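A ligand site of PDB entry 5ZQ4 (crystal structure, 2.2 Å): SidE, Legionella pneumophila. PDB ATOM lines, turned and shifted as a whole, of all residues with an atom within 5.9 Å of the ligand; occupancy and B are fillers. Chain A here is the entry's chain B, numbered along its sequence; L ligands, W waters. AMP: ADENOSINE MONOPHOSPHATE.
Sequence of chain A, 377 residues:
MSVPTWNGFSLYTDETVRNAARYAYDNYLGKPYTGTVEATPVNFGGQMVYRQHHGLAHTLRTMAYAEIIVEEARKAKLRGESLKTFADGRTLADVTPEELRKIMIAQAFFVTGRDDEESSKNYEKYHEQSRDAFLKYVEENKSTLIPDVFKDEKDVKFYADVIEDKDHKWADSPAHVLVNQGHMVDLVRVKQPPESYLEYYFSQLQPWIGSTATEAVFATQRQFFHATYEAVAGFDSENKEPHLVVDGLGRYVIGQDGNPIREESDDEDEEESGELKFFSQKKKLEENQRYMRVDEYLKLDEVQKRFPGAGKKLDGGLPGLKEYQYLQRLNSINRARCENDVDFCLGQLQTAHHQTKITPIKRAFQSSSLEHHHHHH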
ATOM      1  N   HIS A  54      16.352  14.126 -18.531  1.00  0.00           N
ATOM      2  CA  HIS A  54      16.774  15.434 -18.067  1.00  0.00           C
ATOM      3  C   HIS A  54      15.565  16.206 -17.559  1.00  0.00           C
ATOM      4  O   HIS A  54      15.213  17.254 -18.093  1.00  0.00           O
ATOM      5  CB  HIS A  54      17.493  16.196 -19.190  1.00  0.00           C
ATOM      6  CG  HIS A  54      18.837  15.644 -19.530  1.00  0.00           C
ATOM      7  ND1 HIS A  54      19.057  14.846 -20.634  1.00  0.00           N
ATOM      8  CD2 HIS A  54      20.030  15.728 -18.885  1.00  0.00           C
ATOM      9  CE1 HIS A  54      20.325  14.477 -20.668  1.00  0.00           C
ATOM     10  NE2 HIS A  54      20.936  15.003 -19.628  1.00  0.00           N
ATOM     11  N   PHE A 110      19.577  24.509 -15.712  1.00  0.00           N
ATOM     12  CA  PHE A 110      20.637  24.069 -16.631  1.00  0.00           C
ATOM     13  C   PHE A 110      20.153  23.195 -17.804  1.00  0.00           C
ATOM     14  O   PHE A 110      20.812  23.162 -18.842  1.00  0.00           O
ATOM     15  CB  PHE A 110      21.734  23.350 -15.828  1.00  0.00           C
ATOM     16  CG  PHE A 110      23.033  23.171 -16.569  1.00  0.00           C
ATOM     17  CD1 PHE A 110      23.724  24.268 -17.078  1.00  0.00           C
ATOM     18  CD2 PHE A 110      23.570  21.903 -16.764  1.00  0.00           C
ATOM     19  CE1 PHE A 110      24.936  24.102 -17.753  1.00  0.00           C
ATOM     20  CE2 PHE A 110      24.769  21.732 -17.442  1.00  0.00           C
ATOM     21  CZ  PHE A 110      25.456  22.834 -17.942  1.00  0.00           C
ATOM     22  N   ARG A 114      16.248  22.501 -23.143  1.00  0.00           N
ATOM     23  CA  ARG A 114      16.177  21.357 -24.047  1.00  0.00           C
ATOM     24  C   ARG A 114      14.817  21.194 -24.718  1.00  0.00           C
ATOM     25  O   ARG A 114      13.784  21.320 -24.072  1.00  0.00           O
ATOM     26  CB  ARG A 114      16.527  20.068 -23.300  1.00  0.00           C
ATOM     27  CG  ARG A 114      18.008  19.792 -23.169  1.00  0.00           C
ATOM     28  CD  ARG A 114      18.220  18.299 -22.894  1.00  0.00           C
ATOM     29  NE  ARG A 114      19.539  18.041 -22.314  1.00  0.00           N
ATOM     30  CZ  ARG A 114      20.603  17.673 -23.019  1.00  0.00           C
ATOM     31  NH1 ARG A 114      20.511  17.507 -24.342  1.00  0.00           N
ATOM     32  NH2 ARG A 114      21.763  17.454 -22.402  1.00  0.00           N
ATOM     33  N   TYR A 123      23.495  21.824 -29.063  1.00  0.00           N
ATOM     34  CA  TYR A 123      24.161  22.226 -27.822  1.00  0.00           C
ATOM     35  C   TYR A 123      23.976  23.715 -27.517  1.00  0.00           C
ATOM     36  O   TYR A 123      23.507  24.073 -26.436  1.00  0.00           O
ATOM     37  CB  TYR A 123      25.657  21.895 -27.882  1.00  0.00           C
ATOM     38  CG  TYR A 123      26.373  22.054 -26.549  1.00  0.00           C
ATOM     39  CD1 TYR A 123      26.900  23.277 -26.156  1.00  0.00           C
ATOM     40  CD2 TYR A 123      26.507  20.973 -25.682  1.00  0.00           C
ATOM     41  CE1 TYR A 123      27.545  23.421 -24.927  1.00  0.00           C
ATOM     42  CE2 TYR A 123      27.150  21.105 -24.459  1.00  0.00           C
ATOM     43  CZ  TYR A 123      27.665  22.331 -24.084  1.00  0.00           C
ATOM     44  OH  TYR A 123      28.298  22.455 -22.873  1.00  0.00           O
ATOM     45  N   HIS A 127      21.431  25.456 -24.629  1.00  0.00           N
ATOM     46  CA  HIS A 127      22.125  26.187 -23.575  1.00  0.00           C
ATOM     47  C   HIS A 127      21.703  27.650 -23.526  1.00  0.00           C
ATOM     48  O   HIS A 127      21.489  28.206 -22.444  1.00  0.00           O
ATOM     49  CB  HIS A 127      23.637  26.075 -23.748  1.00  0.00           C
ATOM     50  CG  HIS A 127      24.213  24.839 -23.129  1.00  0.00           C
ATOM     51  ND1 HIS A 127      24.675  24.815 -21.829  1.00  0.00           N
ATOM     52  CD2 HIS A 127      24.391  23.592 -23.614  1.00  0.00           C
ATOM     53  CE1 HIS A 127      25.111  23.606 -21.536  1.00  0.00           C
ATOM     54  NE2 HIS A 127      24.949  22.839 -22.602  1.00  0.00           N
ATOM     55  N   ASP A 165      27.371  28.445 -21.107  1.00  0.00           N
ATOM     56  CA  ASP A 165      28.620  27.737 -21.383  1.00  0.00           C
ATOM     57  C   ASP A 165      29.186  27.997 -22.790  1.00  0.00           C
ATOM     58  O   ASP A 165      29.375  27.065 -23.568  1.00  0.00           O
ATOM     59  CB  ASP A 165      28.436  26.232 -21.185  1.00  0.00           C
ATOM     60  CG  ASP A 165      29.754  25.479 -21.201  1.00  0.00           C
ATOM     61  OD1 ASP A 165      30.685  25.901 -20.481  1.00  0.00           O
ATOM     62  OD2 ASP A 165      29.866  24.474 -21.937  1.00  0.00           O
ATOM     63  N   HIS A 168      32.944  26.597 -22.957  1.00  0.00           N
ATOM     64  CA  HIS A 168      33.120  25.288 -22.315  1.00  0.00           C
ATOM     65  C   HIS A 168      34.231  25.267 -21.260  1.00  0.00           C
ATOM     66  O   HIS A 168      34.932  24.262 -21.119  1.00  0.00           O
ATOM     67  CB  HIS A 168      33.412  24.211 -23.371  1.00  0.00           C
ATOM     68  CG  HIS A 168      32.483  24.269 -24.538  1.00  0.00           C
ATOM     69  ND1 HIS A 168      32.762  24.974 -25.686  1.00  0.00           N
ATOM     70  CD2 HIS A 168      31.253  23.717 -24.732  1.00  0.00           C
ATOM     71  CE1 HIS A 168      31.773  24.852 -26.540  1.00  0.00           C
ATOM     72  NE2 HIS A 168      30.844  24.092 -25.996  1.00  0.00           N
ATOM     73  N   TRP A 170      34.788  24.452 -18.235  1.00  0.00           N
ATOM     74  CA  TRP A 170      34.097  23.717 -17.174  1.00  0.00           C
ATOM     75  C   TRP A 170      34.798  23.783 -15.813  1.00  0.00           C
ATOM     76  O   TRP A 170      34.209  23.432 -14.807  1.00  0.00           O
ATOM     77  CB  TRP A 170      33.907  22.257 -17.579  1.00  0.00           C
ATOM     78  CG  TRP A 170      33.098  22.094 -18.828  1.00  0.00           C
ATOM     79  CD1 TRP A 170      32.189  22.990 -19.338  1.00  0.00           C
ATOM     80  CD2 TRP A 170      33.152  21.008 -19.759  1.00  0.00           C
ATOM     81  NE1 TRP A 170      31.656  22.504 -20.509  1.00  0.00           N
ATOM     82  CE2 TRP A 170      32.228  21.288 -20.798  1.00  0.00           C
ATOM     83  CE3 TRP A 170      33.873  19.813 -19.800  1.00  0.00           C
ATOM     84  CZ2 TRP A 170      32.016  20.418 -21.868  1.00  0.00           C
ATOM     85  CZ3 TRP A 170      33.669  18.947 -20.881  1.00  0.00           C
ATOM     86  CH2 TRP A 170      32.743  19.260 -21.890  1.00  0.00           C
ATOM     87  N   VAL A 177      32.572  24.309 -12.050  1.00  0.00           N
ATOM     88  CA  VAL A 177      32.808  22.924 -11.666  1.00  0.00           C
ATOM     89  C   VAL A 177      31.546  22.260 -11.132  1.00  0.00           C
ATOM     90  O   VAL A 177      31.169  21.152 -11.547  1.00  0.00           O
ATOM     91  CB  VAL A 177      33.939  22.826 -10.624  1.00  0.00           C
ATOM     92  CG1 VAL A 177      34.031  21.393 -10.072  1.00  0.00           C
ATOM     93  CG2 VAL A 177      35.265  23.282 -11.243  1.00  0.00           C
ATOM     94  N   VAL A 179      28.229  23.061 -11.385  1.00  0.00           N
ATOM     95  CA  VAL A 179      27.189  22.900 -12.393  1.00  0.00           C
ATOM     96  C   VAL A 179      27.514  21.786 -13.407  1.00  0.00           C
ATOM     97  O   VAL A 179      26.701  20.906 -13.666  1.00  0.00           O
ATOM     98  CB  VAL A 179      26.941  24.214 -13.160  1.00  0.00           C
ATOM     99  CG1 VAL A 179      26.015  23.986 -14.339  1.00  0.00           C
ATOM    100  CG2 VAL A 179      26.413  25.309 -12.228  1.00  0.00           C
ATOM    101  N   ASN A 180      28.715  21.846 -13.985  1.00  0.00           N
ATOM    102  CA  ASN A 180      29.066  20.907 -15.063  1.00  0.00           C
ATOM    103  C   ASN A 180      29.328  19.483 -14.567  1.00  0.00           C
ATOM    104  O   ASN A 180      28.870  18.519 -15.167  1.00  0.00           O
ATOM    105  CB  ASN A 180      30.273  21.417 -15.837  1.00  0.00           C
ATOM    106  CG  ASN A 180      29.924  22.602 -16.709  1.00  0.00           C
ATOM    107  OD1 ASN A 180      29.302  22.448 -17.760  1.00  0.00           O
ATOM    108  ND2 ASN A 180      30.345  23.804 -16.288  1.00  0.00           N
ATOM    109  N   GLN A 181      30.053  19.349 -13.465  1.00  0.00           N
ATOM    110  CA  GLN A 181      30.315  18.023 -12.911  1.00  0.00           C
ATOM    111  C   GLN A 181      29.073  17.459 -12.206  1.00  0.00           C
ATOM    112  O   GLN A 181      28.848  16.244 -12.238  1.00  0.00           O
ATOM    113  CB  GLN A 181      31.527  18.055 -11.973  1.00  0.00           C
ATOM    114  CG  GLN A 181      32.836  18.321 -12.717  1.00  0.00           C
ATOM    115  CD  GLN A 181      34.018  17.708 -12.004  1.00  0.00           C
ATOM    116  OE1 GLN A 181      33.904  16.654 -11.353  1.00  0.00           O
ATOM    117  NE2 GLN A 181      35.175  18.378 -12.086  1.00  0.00           N
ATOM    118  N   HIS A 183      26.037  17.958 -13.263  1.00  0.00           N
ATOM    119  CA  HIS A 183      25.283  17.487 -14.421  1.00  0.00           C
ATOM    120  C   HIS A 183      25.837  16.165 -14.948  1.00  0.00           C
ATOM    121  O   HIS A 183      25.099  15.244 -15.277  1.00  0.00           O
ATOM    122  CB  HIS A 183      25.328  18.554 -15.519  1.00  0.00           C
ATOM    123  CG  HIS A 183      24.776  18.095 -16.841  1.00  0.00           C
ATOM    124  ND1 HIS A 183      23.464  18.291 -17.198  1.00  0.00           N
ATOM    125  CD2 HIS A 183      25.372  17.489 -17.893  1.00  0.00           C
ATOM    126  CE1 HIS A 183      23.274  17.811 -18.416  1.00  0.00           C
ATOM    127  NE2 HIS A 183      24.409  17.313 -18.852  1.00  0.00           N
ATOM    128  N   MET A 184      27.160  16.086 -14.998  1.00  0.00           N
ATOM    129  CA  MET A 184      27.896  14.954 -15.560  1.00  0.00           C
ATOM    130  C   MET A 184      27.702  13.668 -14.766  1.00  0.00           C
ATOM    131  O   MET A 184      27.390  12.621 -15.316  1.00  0.00           O
ATOM    132  CB  MET A 184      29.385  15.296 -15.635  1.00  0.00           C
ATOM    133  CG  MET A 184      30.284  14.158 -16.071  1.00  0.00           C
ATOM    134  SD  MET A 184      32.064  14.502 -15.893  1.00  0.00           S
ATOM    135  CE  MET A 184      32.288  14.553 -14.120  1.00  0.00           C
ATOM    136  N   LEU A 187      25.086  10.722 -14.803  1.00  0.00           N
ATOM    137  CA  LEU A 187      25.077   9.700 -15.849  1.00  0.00           C
ATOM    138  C   LEU A 187      25.481   8.331 -15.290  1.00  0.00           C
ATOM    139  O   LEU A 187      25.379   7.328 -15.992  1.00  0.00           O
ATOM    140  CB  LEU A 187      26.004  10.112 -16.990  1.00  0.00           C
ATOM    141  CG  LEU A 187      25.455  11.280 -17.826  1.00  0.00           C
ATOM    142  CD1 LEU A 187      26.481  11.806 -18.831  1.00  0.00           C
ATOM    143  CD2 LEU A 187      24.165  10.864 -18.546  1.00  0.00           C
ATOM    144  N   TYR A 200      36.442   7.179 -14.319  1.00  0.00           N
ATOM    145  CA  TYR A 200      36.657   8.412 -15.067  1.00  0.00           C
ATOM    146  C   TYR A 200      36.110   9.614 -14.301  1.00  0.00           C
ATOM    147  O   TYR A 200      36.808  10.618 -14.147  1.00  0.00           O
ATOM    148  CB  TYR A 200      36.016   8.363 -16.448  1.00  0.00           C
ATOM    149  CG  TYR A 200      36.065   9.709 -17.127  1.00  0.00           C
ATOM    150  CD1 TYR A 200      37.255  10.186 -17.679  1.00  0.00           C
ATOM    151  CD2 TYR A 200      34.936  10.516 -17.183  1.00  0.00           C
ATOM    152  CE1 TYR A 200      37.305  11.427 -18.283  1.00  0.00           C
ATOM    153  CE2 TYR A 200      34.979  11.761 -17.792  1.00  0.00           C
ATOM    154  CZ  TYR A 200      36.160  12.209 -18.333  1.00  0.00           C
ATOM    155  OH  TYR A 200      36.205  13.442 -18.934  1.00  0.00           O
ATOM    156  N   GLN A 204      37.840  13.059 -12.459  1.00  0.00           N
ATOM    157  CA  GLN A 204      37.474  14.452 -12.755  1.00  0.00           C
ATOM    158  C   GLN A 204      37.183  15.251 -11.480  1.00  0.00           C
ATOM    159  O   GLN A 204      37.495  16.438 -11.424  1.00  0.00           O
ATOM    160  CB  GLN A 204      36.267  14.503 -13.697  1.00  0.00           C
ATOM    161  CG  GLN A 204      36.536  13.914 -15.073  1.00  0.00           C
ATOM    162  CD  GLN A 204      37.749  14.528 -15.754  1.00  0.00           C
ATOM    163  OE1 GLN A 204      37.689  15.660 -16.252  1.00  0.00           O
ATOM    164  NE2 GLN A 204      38.847  13.790 -15.756  1.00  0.00           N
HETATM  165  P   AMP L   1      25.424  15.045 -21.685  1.00  0.00           P
HETATM  166  O1P AMP L   1      24.522  14.184 -20.820  1.00  0.00           O
HETATM  167  O2P AMP L   1      24.656  16.019 -22.557  1.00  0.00           O
HETATM  168  O3P AMP L   1      26.540  14.306 -22.364  1.00  0.00           O
HETATM  169  O5' AMP L   1      26.258  16.017 -20.719  1.00  0.00           O
HETATM  170  C5' AMP L   1      27.501  16.577 -21.126  1.00  0.00           C
HETATM  171  C4' AMP L   1      27.922  17.712 -20.211  1.00  0.00           C
HETATM  172  O4' AMP L   1      28.521  17.186 -19.001  1.00  0.00           O
HETATM  173  C3' AMP L   1      28.980  18.673 -20.735  1.00  0.00           C
HETATM  174  O3' AMP L   1      28.484  19.624 -21.666  1.00  0.00           O
HETATM  175  C2' AMP L   1      29.505  19.299 -19.459  1.00  0.00           C
HETATM  176  O2' AMP L   1      28.588  20.246 -18.947  1.00  0.00           O
HETATM  177  C1' AMP L   1      29.504  18.091 -18.522  1.00  0.00           C
HETATM  178  N9  AMP L   1      30.818  17.416 -18.530  1.00  0.00           N
HETATM  179  C8  AMP L   1      31.150  16.367 -19.301  1.00  0.00           C
HETATM  180  N7  AMP L   1      32.431  15.993 -19.057  1.00  0.00           N
HETATM  181  C5  AMP L   1      32.934  16.811 -18.120  1.00  0.00           C
HETATM  182  C6  AMP L   1      34.219  16.945 -17.416  1.00  0.00           C
HETATM  183  N6  AMP L   1      35.233  16.084 -17.709  1.00  0.00           N
HETATM  184  N1  AMP L   1      34.325  17.947 -16.499  1.00  0.00           N
HETATM  185  C2  AMP L   1      33.313  18.791 -16.222  1.00  0.00           C
HETATM  186  N3  AMP L   1      32.109  18.712 -16.826  1.00  0.00           N
HETATM  187  C4  AMP L   1      31.865  17.758 -17.773  1.00  0.00           C
HETATM  188  O   HOH W   1      36.858  19.162 -15.490  1.00  0.00           O
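O3' of the ligand sits at hydrogen-bond distance from OH of Tyr 123, at 3.1 Å.
NH2 of Arg 114 lies within salt-bridge range of O2P of the ligand (3.2 Å).
An oxygen (O2') of the ligand lies within hydrogen-bond range of the side-chain amide oxygen (OD1) of Asn 180 (2.6 Å).
OE1 of Gln 204 sits at hydrogen-bond distance from N6 of the ligand, 2.9 Å away.
A nitrogen (N6) of the ligand sits at hydrogen-bond distance from the side-chain hydroxyl of Tyr 200, 3.1 Å away.
An oxygen (O5') of the ligand lies within hydrogen-bond range of a ring nitrogen (NE2) of His 183 (2.9 Å).
The side-chain hydroxyl of Tyr 123 lies within hydrogen-bond range of the side-chain carboxylate of Asp 165 (2.7 Å).
The side-chain carboxylate of Asp 165 sits at hydrogen-bond distance from the indole nitrogen of Trp 170 (3.0 Å).
NE2 of His 127 sits close to OH of Tyr 123 (3.4 Å).
The backbone carbonyl oxygen of Gln 204 sits at hydrogen-bond distance from the side-chain amide nitrogen of Gln 181 (3.1 Å).
O of Trp 170 is in hydrogen-bond range of N of Val 177.
A nitrogen (N7) of the ligand sits close to the side-chain sulfur (SD) of Met 184.
Merely in contact with the ligand: His 54, Trp 170, Gln 181 and Leu 187.
Hydrophobic or aromatic side chains within 4 Å of the ligand: Tyr 123, Trp 170, His 183, Met 184 and Leu 187.
Within 4 Å of the ligand: His 54, Arg 114, Tyr 123, Trp 170, Asn 180, Gln 181, His 183, Met 184, Leu 187, Tyr 200 and Gln 204.
Along chain A the residues within 4 Å of the ligand span positions 54 to 204.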
